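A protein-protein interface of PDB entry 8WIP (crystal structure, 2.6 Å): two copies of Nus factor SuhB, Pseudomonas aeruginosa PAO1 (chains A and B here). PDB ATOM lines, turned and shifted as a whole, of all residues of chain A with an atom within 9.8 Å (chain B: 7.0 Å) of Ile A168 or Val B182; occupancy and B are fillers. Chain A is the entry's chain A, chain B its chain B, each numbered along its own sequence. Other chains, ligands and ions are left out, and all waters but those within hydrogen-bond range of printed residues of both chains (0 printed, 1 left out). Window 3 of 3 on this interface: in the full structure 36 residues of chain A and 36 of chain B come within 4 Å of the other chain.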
ATOM      1  N   PHE A 161      -5.614  -4.445  15.780  1.00  0.00           N
ATOM      2  CA  PHE A 161      -5.510  -3.338  16.733  1.00  0.00           C
ATOM      3  C   PHE A 161      -6.843  -3.060  17.447  1.00  0.00           C
ATOM      4  O   PHE A 161      -7.902  -3.151  16.822  1.00  0.00           O
ATOM      5  CB  PHE A 161      -5.016  -2.076  16.050  1.00  0.00           C
ATOM      6  CG  PHE A 161      -4.528  -1.038  17.018  1.00  0.00           C
ATOM      7  CD1 PHE A 161      -3.378  -1.253  17.770  1.00  0.00           C
ATOM      8  CD2 PHE A 161      -5.229   0.136  17.193  1.00  0.00           C
ATOM      9  CE1 PHE A 161      -2.932  -0.297  18.672  1.00  0.00           C
ATOM     10  CE2 PHE A 161      -4.797   1.088  18.085  1.00  0.00           C
ATOM     11  CZ  PHE A 161      -3.646   0.872  18.831  1.00  0.00           C
ATOM     12  N   PRO A 162      -6.844  -2.701  18.737  1.00  0.00           N
ATOM     13  CA  PRO A 162      -8.114  -2.279  19.376  1.00  0.00           C
ATOM     14  C   PRO A 162      -8.334  -0.819  18.993  1.00  0.00           C
ATOM     15  O   PRO A 162      -7.525   0.052  19.327  1.00  0.00           O
ATOM     16  CB  PRO A 162      -7.846  -2.459  20.873  1.00  0.00           C
ATOM     17  CG  PRO A 162      -6.406  -2.293  21.019  1.00  0.00           C
ATOM     18  CD  PRO A 162      -5.726  -2.649  19.696  1.00  0.00           C
ATOM     19  N   PHE A 163      -9.469  -0.528  18.389  1.00  0.00           N
ATOM     20  CA  PHE A 163      -9.665   0.764  17.735  1.00  0.00           C
ATOM     21  C   PHE A 163     -10.234   1.851  18.634  1.00  0.00           C
ATOM     22  O   PHE A 163     -10.294   3.012  18.205  1.00  0.00           O
ATOM     23  CB  PHE A 163     -10.431   0.621  16.436  1.00  0.00           C
ATOM     24  CG  PHE A 163      -9.504   0.621  15.242  1.00  0.00           C
ATOM     25  CD1 PHE A 163      -9.083   1.814  14.675  1.00  0.00           C
ATOM     26  CD2 PHE A 163      -8.995  -0.573  14.731  1.00  0.00           C
ATOM     27  CE1 PHE A 163      -8.218   1.822  13.596  1.00  0.00           C
ATOM     28  CE2 PHE A 163      -8.114  -0.560  13.654  1.00  0.00           C
ATOM     29  CZ  PHE A 163      -7.726   0.643  13.094  1.00  0.00           C
ATOM     30  N   ARG A 164     -10.677   1.516  19.837  1.00  0.00           N
ATOM     31  CA  ARG A 164     -11.297   2.488  20.711  1.00  0.00           C
ATOM     32  C   ARG A 164     -10.214   3.439  21.243  1.00  0.00           C
ATOM     33  O   ARG A 164      -9.030   3.100  21.334  1.00  0.00           O
ATOM     34  CB  ARG A 164     -12.024   1.798  21.855  1.00  0.00           C
ATOM     35  CG  ARG A 164     -11.120   1.074  22.826  1.00  0.00           C
ATOM     36  CD  ARG A 164     -11.188  -0.412  22.578  1.00  0.00           C
ATOM     37  NE  ARG A 164     -10.534  -1.140  23.658  1.00  0.00           N
ATOM     38  CZ  ARG A 164     -10.400  -2.455  23.696  1.00  0.00           C
ATOM     39  NH1 ARG A 164     -10.854  -3.218  22.719  1.00  0.00           N
ATOM     40  NH2 ARG A 164      -9.807  -3.016  24.749  1.00  0.00           N
ATOM     41  N   ASP A 165     -10.672   4.625  21.654  1.00  0.00           N
ATOM     42  CA  ASP A 165      -9.826   5.676  22.229  1.00  0.00           C
ATOM     43  C   ASP A 165      -8.939   5.232  23.400  1.00  0.00           C
ATOM     44  O   ASP A 165      -7.742   5.568  23.396  1.00  0.00           O
ATOM     45  CB  ASP A 165     -10.766   6.841  22.619  1.00  0.00           C
ATOM     46  CG  ASP A 165     -10.165   7.862  23.626  1.00  0.00           C
ATOM     47  OD1 ASP A 165      -9.159   7.609  24.309  1.00  0.00           O
ATOM     48  OD2 ASP A 165     -10.733   8.982  23.741  1.00  0.00           O
ATOM     49  N   ASN A 166      -9.441   4.437  24.368  1.00  0.00           N
ATOM     50  CA  ASN A 166      -8.517   4.164  25.493  1.00  0.00           C
ATOM     51  C   ASN A 166      -7.297   3.285  25.137  1.00  0.00           C
ATOM     52  O   ASN A 166      -6.540   2.937  26.065  1.00  0.00           O
ATOM     53  CB  ASN A 166      -9.225   3.547  26.719  1.00  0.00           C
ATOM     54  CG  ASN A 166      -9.990   2.274  26.406  1.00  0.00           C
ATOM     55  OD1 ASN A 166      -9.501   1.385  25.693  1.00  0.00           O
ATOM     56  ND2 ASN A 166     -11.174   2.145  27.007  1.00  0.00           N
ATOM     57  N   GLN A 167      -7.101   2.863  23.878  1.00  0.00           N
ATOM     58  CA  GLN A 167      -5.864   2.173  23.495  1.00  0.00           C
ATOM     59  C   GLN A 167      -4.909   3.020  22.631  1.00  0.00           C
ATOM     60  O   GLN A 167      -3.867   2.500  22.192  1.00  0.00           O
ATOM     61  CB  GLN A 167      -6.177   0.821  22.833  1.00  0.00           C
ATOM     62  CG  GLN A 167      -5.347  -0.352  23.464  1.00  0.00           C
ATOM     63  CD  GLN A 167      -5.810  -0.818  24.857  1.00  0.00           C
ATOM     64  OE1 GLN A 167      -6.992  -0.714  25.200  1.00  0.00           O
ATOM     65  NE2 GLN A 167      -4.875  -1.372  25.645  1.00  0.00           N
ATOM     66  N   ILE A 168      -5.247   4.299  22.385  1.00  0.00           N
ATOM     67  CA  ILE A 168      -4.540   5.170  21.426  1.00  0.00           C
ATOM     68  C   ILE A 168      -3.057   5.330  21.861  1.00  0.00           C
ATOM     69  O   ILE A 168      -2.122   5.224  21.037  1.00  0.00           O
ATOM     70  CB  ILE A 168      -5.317   6.501  21.290  1.00  0.00           C
ATOM     71  CG1 ILE A 168      -4.801   7.395  20.150  1.00  0.00           C
ATOM     72  CG2 ILE A 168      -5.004   7.384  22.589  1.00  0.00           C
ATOM     73  CD1 ILE A 168      -4.835   6.699  18.623  1.00  0.00           C
ATOM     74  N   ASP A 169      -2.827   5.456  23.181  1.00  0.00           N
ATOM     75  CA  ASP A 169      -1.535   5.615  23.857  1.00  0.00           C
ATOM     76  C   ASP A 169      -0.638   4.384  23.708  1.00  0.00           C
ATOM     77  O   ASP A 169       0.515   4.431  24.154  1.00  0.00           O
ATOM     78  CB  ASP A 169      -1.711   5.889  25.370  1.00  0.00           C
ATOM     79  CG  ASP A 169      -2.846   6.877  25.706  1.00  0.00           C
ATOM     80  OD1 ASP A 169      -3.999   6.409  25.835  1.00  0.00           O
ATOM     81  OD2 ASP A 169      -2.596   8.096  25.907  1.00  0.00           O
ATOM     82  N   ASN A 170      -1.151   3.284  23.150  1.00  0.00           N
ATOM     83  CA  ASN A 170      -0.385   2.066  22.889  1.00  0.00           C
ATOM     84  C   ASN A 170      -0.001   1.916  21.420  1.00  0.00           C
ATOM     85  O   ASN A 170       0.743   0.985  21.080  1.00  0.00           O
ATOM     86  CB  ASN A 170      -1.125   0.825  23.405  1.00  0.00           C
ATOM     87  CG  ASN A 170      -1.265   0.824  24.932  1.00  0.00           C
ATOM     88  OD1 ASN A 170      -0.579   1.578  25.623  1.00  0.00           O
ATOM     89  ND2 ASN A 170      -2.199   0.019  25.451  1.00  0.00           N
ATOM     90  N   LEU A 171      -0.485   2.812  20.549  1.00  0.00           N
ATOM     91  CA  LEU A 171      -0.271   2.687  19.105  1.00  0.00           C
ATOM     92  C   LEU A 171       1.196   2.515  18.748  1.00  0.00           C
ATOM     93  O   LEU A 171       1.549   1.588  18.012  1.00  0.00           O
ATOM     94  CB  LEU A 171      -0.777   3.942  18.391  1.00  0.00           C
ATOM     95  CG  LEU A 171      -1.203   3.871  16.926  1.00  0.00           C
ATOM     96  CD1 LEU A 171      -1.861   2.567  16.507  1.00  0.00           C
ATOM     97  CD2 LEU A 171      -2.006   5.120  16.558  1.00  0.00           C
ATOM     98  N   ASP A 172       2.068   3.406  19.234  1.00  0.00           N
ATOM     99  CA  ASP A 172       3.480   3.250  18.903  1.00  0.00           C
ATOM    100  C   ASP A 172       3.990   1.889  19.336  1.00  0.00           C
ATOM    101  O   ASP A 172       4.636   1.191  18.543  1.00  0.00           O
ATOM    102  CB  ASP A 172       4.315   4.374  19.504  1.00  0.00           C
ATOM    103  CG  ASP A 172       4.097   5.695  18.776  1.00  0.00           C
ATOM    104  OD1 ASP A 172       5.066   6.209  18.140  1.00  0.00           O
ATOM    105  OD2 ASP A 172       2.928   6.173  18.772  1.00  0.00           O
ATOM    106  N   ASN A 173       3.645   1.457  20.557  1.00  0.00           N
ATOM    107  CA  ASN A 173       4.034   0.115  20.977  1.00  0.00           C
ATOM    108  C   ASN A 173       3.607  -0.913  19.934  1.00  0.00           C
ATOM    109  O   ASN A 173       4.433  -1.679  19.421  1.00  0.00           O
ATOM    110  CB  ASN A 173       3.408  -0.182  22.334  1.00  0.00           C
ATOM    111  CG  ASN A 173       4.005   0.670  23.430  1.00  0.00           C
ATOM    112  OD1 ASN A 173       3.323   1.521  24.015  1.00  0.00           O
ATOM    113  ND2 ASN A 173       5.279   0.441  23.727  1.00  0.00           N
ATOM    114  N   TYR A 174       2.331  -0.884  19.542  1.00  0.00           N
ATOM    115  CA  TYR A 174       1.864  -1.827  18.536  1.00  0.00           C
ATOM    116  C   TYR A 174       2.637  -1.678  17.248  1.00  0.00           C
ATOM    117  O   TYR A 174       3.152  -2.660  16.695  1.00  0.00           O
ATOM    118  CB  TYR A 174       0.375  -1.658  18.286  1.00  0.00           C
ATOM    119  CG  TYR A 174      -0.091  -2.605  17.211  1.00  0.00           C
ATOM    120  CD1 TYR A 174      -0.458  -3.926  17.490  1.00  0.00           C
ATOM    121  CD2 TYR A 174      -0.192  -2.155  15.898  1.00  0.00           C
ATOM    122  CE1 TYR A 174      -0.890  -4.774  16.474  1.00  0.00           C
ATOM    123  CE2 TYR A 174      -0.620  -2.988  14.887  1.00  0.00           C
ATOM    124  CZ  TYR A 174      -0.975  -4.291  15.181  1.00  0.00           C
ATOM    125  OH  TYR A 174      -1.391  -5.090  14.150  1.00  0.00           O
ATOM    126  N   LEU A 175       2.782  -0.436  16.793  1.00  0.00           N
ATOM    127  CA  LEU A 175       3.446  -0.194  15.528  1.00  0.00           C
ATOM    128  C   LEU A 175       4.897  -0.585  15.609  1.00  0.00           C
ATOM    129  O   LEU A 175       5.491  -0.890  14.579  1.00  0.00           O
ATOM    130  CB  LEU A 175       3.286   1.262  15.091  1.00  0.00           C
ATOM    131  CG  LEU A 175       1.851   1.563  14.654  1.00  0.00           C
ATOM    132  CD1 LEU A 175       1.753   2.993  14.178  1.00  0.00           C
ATOM    133  CD2 LEU A 175       1.398   0.603  13.571  1.00  0.00           C
ATOM    134  N   ARG A 190      -4.784  -8.459   9.193  1.00  0.00           N
ATOM    135  CA  ARG A 190      -5.736  -7.873  10.140  1.00  0.00           C
ATOM    136  C   ARG A 190      -7.120  -8.039   9.520  1.00  0.00           C
ATOM    137  O   ARG A 190      -7.582  -7.201   8.746  1.00  0.00           O
ATOM    138  CB  ARG A 190      -5.430  -6.391  10.379  1.00  0.00           C
ATOM    139  CG  ARG A 190      -6.029  -5.813  11.682  1.00  0.00           C
ATOM    140  CD  ARG A 190      -5.307  -4.584  12.288  1.00  0.00           C
ATOM    141  NE  ARG A 190      -3.872  -4.544  12.005  1.00  0.00           N
ATOM    142  CZ  ARG A 190      -3.306  -3.771  11.088  1.00  0.00           C
ATOM    143  NH1 ARG A 190      -4.026  -2.935  10.348  1.00  0.00           N
ATOM    144  NH2 ARG A 190      -1.974  -3.808  10.937  1.00  0.00           N
ATOM    145  N   PHE A 212      -3.492  -7.383  21.624  1.00  0.00           N
ATOM    146  CA  PHE A 212      -3.909  -6.927  22.944  1.00  0.00           C
ATOM    147  C   PHE A 212      -5.210  -6.134  22.878  1.00  0.00           C
ATOM    148  O   PHE A 212      -5.680  -5.752  21.803  1.00  0.00           O
ATOM    149  CB  PHE A 212      -2.813  -6.066  23.594  1.00  0.00           C
ATOM    150  CG  PHE A 212      -2.509  -4.814  22.831  1.00  0.00           C
ATOM    151  CD1 PHE A 212      -3.300  -3.684  22.965  1.00  0.00           C
ATOM    152  CD2 PHE A 212      -1.429  -4.774  21.956  1.00  0.00           C
ATOM    153  CE1 PHE A 212      -3.025  -2.537  22.235  1.00  0.00           C
ATOM    154  CE2 PHE A 212      -1.141  -3.633  21.236  1.00  0.00           C
ATOM    155  CZ  PHE A 212      -1.949  -2.509  21.377  1.00  0.00           C
ATOM    156  N   MET B 177       1.094   6.890   7.646  1.00  0.00           N
ATOM    157  CA  MET B 177      -0.264   6.929   7.116  1.00  0.00           C
ATOM    158  C   MET B 177      -1.203   6.266   8.121  1.00  0.00           C
ATOM    159  O   MET B 177      -2.094   6.909   8.688  1.00  0.00           O
ATOM    160  CB  MET B 177      -0.299   6.250   5.735  1.00  0.00           C
ATOM    161  CG  MET B 177       0.519   7.009   4.622  1.00  0.00           C
ATOM    162  SD  MET B 177       0.885   6.339   2.921  1.00  0.00           S
ATOM    163  CE  MET B 177       0.765   4.552   3.111  1.00  0.00           C
ATOM    164  N   PHE B 178      -0.937   4.991   8.418  1.00  0.00           N
ATOM    165  CA  PHE B 178      -1.714   4.236   9.396  1.00  0.00           C
ATOM    166  C   PHE B 178      -1.963   5.053  10.662  1.00  0.00           C
ATOM    167  O   PHE B 178      -3.102   5.138  11.142  1.00  0.00           O
ATOM    168  CB  PHE B 178      -1.011   2.912   9.715  1.00  0.00           C
ATOM    169  CG  PHE B 178      -1.828   1.974  10.580  1.00  0.00           C
ATOM    170  CD1 PHE B 178      -2.767   1.127  10.000  1.00  0.00           C
ATOM    171  CD2 PHE B 178      -1.664   1.941  11.959  1.00  0.00           C
ATOM    172  CE1 PHE B 178      -3.535   0.269  10.784  1.00  0.00           C
ATOM    173  CE2 PHE B 178      -2.432   1.077  12.754  1.00  0.00           C
ATOM    174  CZ  PHE B 178      -3.366   0.241  12.164  1.00  0.00           C
ATOM    175  N   ARG B 179      -0.918   5.684  11.210  1.00  0.00           N
ATOM    176  CA  ARG B 179      -1.089   6.379  12.487  1.00  0.00           C
ATOM    177  C   ARG B 179      -2.163   7.443  12.380  1.00  0.00           C
ATOM    178  O   ARG B 179      -3.121   7.464  13.168  1.00  0.00           O
ATOM    179  CB  ARG B 179       0.215   7.073  12.888  1.00  0.00           C
ATOM    180  CG  ARG B 179       1.240   6.246  13.567  1.00  0.00           C
ATOM    181  CD  ARG B 179       2.644   6.855  13.381  1.00  0.00           C
ATOM    182  NE  ARG B 179       3.674   5.947  13.875  1.00  0.00           N
ATOM    183  CZ  ARG B 179       4.182   5.988  15.099  1.00  0.00           C
ATOM    184  NH1 ARG B 179       3.776   6.886  15.987  1.00  0.00           N
ATOM    185  NH2 ARG B 179       5.088   5.082  15.456  1.00  0.00           N
ATOM    186  N   SER B 180      -2.081   8.265  11.332  1.00  0.00           N
ATOM    187  CA  SER B 180      -3.000   9.383  11.232  1.00  0.00           C
ATOM    188  C   SER B 180      -4.443   8.938  11.035  1.00  0.00           C
ATOM    189  O   SER B 180      -5.352   9.768  11.162  1.00  0.00           O
ATOM    190  CB  SER B 180      -2.548  10.295  10.096  1.00  0.00           C
ATOM    191  OG  SER B 180      -2.561   9.584   8.871  1.00  0.00           O
ATOM    192  N   LEU B 181      -4.675   7.662  10.726  1.00  0.00           N
ATOM    193  CA  LEU B 181      -6.022   7.168  10.511  1.00  0.00           C
ATOM    194  C   LEU B 181      -6.625   6.469  11.733  1.00  0.00           C
ATOM    195  O   LEU B 181      -7.840   6.220  11.746  1.00  0.00           O
ATOM    196  CB  LEU B 181      -5.990   6.212   9.317  1.00  0.00           C
ATOM    197  CG  LEU B 181      -5.675   6.937   8.004  1.00  0.00           C
ATOM    198  CD1 LEU B 181      -5.298   5.936   6.942  1.00  0.00           C
ATOM    199  CD2 LEU B 181      -6.815   7.783   7.515  1.00  0.00           C
ATOM    200  N   VAL B 182      -5.825   6.185  12.773  1.00  0.00           N
ATOM    201  CA  VAL B 182      -6.307   5.313  13.852  1.00  0.00           C
ATOM    202  C   VAL B 182      -7.356   6.004  14.725  1.00  0.00           C
ATOM    203  O   VAL B 182      -8.291   5.362  15.225  1.00  0.00           O
ATOM    204  CB  VAL B 182      -5.107   4.787  14.670  1.00  0.00           C
ATOM    205  CG1 VAL B 182      -5.548   4.147  15.995  1.00  0.00           C
ATOM    206  CG2 VAL B 182      -4.305   3.772  13.832  1.00  0.00           C
ATOM    207  N   GLY B 183      -7.215   7.312  14.939  1.00  0.00           N
ATOM    208  CA  GLY B 183      -8.144   8.020  15.814  1.00  0.00           C
ATOM    209  C   GLY B 183      -9.573   8.010  15.299  1.00  0.00           C
ATOM    210  O   GLY B 183     -10.514   7.743  16.048  1.00  0.00           O
ATOM    211  N   GLN B 184      -9.764   8.415  14.039  1.00  0.00           N
ATOM    212  CA  GLN B 184     -11.111   8.607  13.497  1.00  0.00           C
ATOM    213  C   GLN B 184     -11.826   7.319  13.103  1.00  0.00           C
ATOM    214  O   GLN B 184     -13.042   7.199  13.306  1.00  0.00           O
ATOM    215  CB  GLN B 184     -11.053   9.495  12.267  1.00  0.00           C
ATOM    216  CG  GLN B 184     -11.156  10.949  12.553  1.00  0.00           C
ATOM    217  CD  GLN B 184     -11.366  11.710  11.274  1.00  0.00           C
ATOM    218  OE1 GLN B 184     -10.605  11.546  10.300  1.00  0.00           O
ATOM    219  NE2 GLN B 184     -12.407  12.541  11.252  1.00  0.00           N
ATOM    220  N   THR B 185     -11.109   6.386  12.483  1.00  0.00           N
ATOM    221  CA  THR B 185     -11.721   5.219  11.866  1.00  0.00           C
ATOM    222  C   THR B 185     -12.153   4.185  12.898  1.00  0.00           C
ATOM    223  O   THR B 185     -11.663   4.158  14.025  1.00  0.00           O
ATOM    224  CB  THR B 185     -10.764   4.580  10.852  1.00  0.00           C
ATOM    225  OG1 THR B 185      -9.580   4.163  11.524  1.00  0.00           O
ATOM    226  CG2 THR B 185     -10.403   5.548   9.750  1.00  0.00           C
ATOM    227  N   ALA B 186     -13.118   3.348  12.497  1.00  0.00           N
ATOM    228  CA  ALA B 186     -13.509   2.177  13.268  1.00  0.00           C
ATOM    229  C   ALA B 186     -12.582   0.997  13.038  1.00  0.00           C
ATOM    230  O   ALA B 186     -12.544   0.078  13.864  1.00  0.00           O
ATOM    231  CB  ALA B 186     -14.933   1.761  12.907  1.00  0.00           C
ATOM    232  N   GLY B 187     -11.877   0.972  11.915  1.00  0.00           N
ATOM    233  CA  GLY B 187     -10.937  -0.095  11.669  1.00  0.00           C
ATOM    234  C   GLY B 187     -10.214   0.074  10.346  1.00  0.00           C
ATOM    235  O   GLY B 187     -10.707   0.715   9.404  1.00  0.00           O
ATOM    236  N   ILE B 188      -9.062  -0.573  10.278  1.00  0.00           N
ATOM    237  CA  ILE B 188      -8.278  -0.705   9.061  1.00  0.00           C
ATOM    238  C   ILE B 188      -8.019  -2.194   8.924  1.00  0.00           C
ATOM    239  O   ILE B 188      -7.577  -2.850   9.877  1.00  0.00           O
ATOM    240  CB  ILE B 188      -6.982   0.125   9.086  1.00  0.00           C
ATOM    241  CG1 ILE B 188      -7.319   1.582   9.448  1.00  0.00           C
ATOM    242  CG2 ILE B 188      -6.289   0.056   7.739  1.00  0.00           C
ATOM    243  CD1 ILE B 188      -6.141   2.500   9.604  1.00  0.00           C
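OG1 of Thr B185 lies within hydrogen-bond range of O of Leu B181 (2.7 Å).
The side-chain hydroxyl (OH) of Tyr A174 is in hydrogen-bond range of the guanidinium group (NE) of Arg A190, 3.3 Å away.
No position is printed for both chains.
The guanidinium group (NH1) of Arg B179 lies within salt-bridge range of the side-chain carboxylate (OD1) of Asp A172 (2.6 Å).
Of the 12 printed residues of chain B, 7 touch a printed residue of chain A.
Printed residues of chain B that touch a printed residue of chain A: Phe B178, Arg B179, Val B182, Thr B185, Ala B186, Gly B187 and Ile B188.
Hydrophobic or aromatic side chains of chain B within 4 Å of the printed part of chain A: Phe B178, Val B182 and Ile B188.
Among the printed residues, 13 pairs touch across the chains.
Among the printed residues, Asp or Glu carboxylates within 4 Å of a Lys or Arg side-chain nitrogen of the other chain: Asp A172 with Arg B179 (2.6 Å).
Phe A161 touches Val B182.
Phe A163 touches Val B182 (CD1 to O, 3.7 Å).
CE1 of Phe A163 touches OG1 of Thr B185, 3.4 Å away.
Phe A163 touches Ala B186 (CB to O, 3.4 Å).
CE2 of Phe A163 touches CA of Gly B187 (3.5 Å).
Val B182 touches Leu A171 (CB to CD2, 3.6 Å).
Leu A175 touches Phe B178 (CD2 to CD2, 3.7 Å).
CD1 of Leu A175 touches CG of Arg B179 (3.3 Å).
CE1 of Phe B178 touches NH1 of Arg A190, 3.3 Å away.
NH1 of Arg A190 touches O of Ile B188, 3.6 Å away.
Of the printed residues of chain B, Phe A163 touches Val B182, Thr B185, Ala B186, Gly B187 and Ile B188.
Arg A164 touches none of the printed residues of chain B.
Asp A165 touches none of the printed residues of chain B.
Ile A168 touches just one residue of chain B: Val B182 (3.7 Å).
Of the printed residues of chain B, Leu A171 touches Val B182.
Of the printed residues of chain A, Phe B178 touches Leu A175 (3.7 Å) and Arg A190 (3.3 Å).
Of the printed residues of chain A, Arg B179 touches Asp A172 and Leu A175.
Of chain A, only Phe A161 (3.8 Å), Phe A163 (3.7 Å), Ile A168 (3.7 Å) and Leu A171 (3.6 Å) come within 4 Å of Val B182.
Thr B185 touches just one residue of chain A: Phe A163.
The nearest residue of chain B that does not touch Ile A168 is Gly B183 (4.4 Å).
The nearest residue of chain A that does not touch Val B182 is Pro A162 (5.6 Å).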
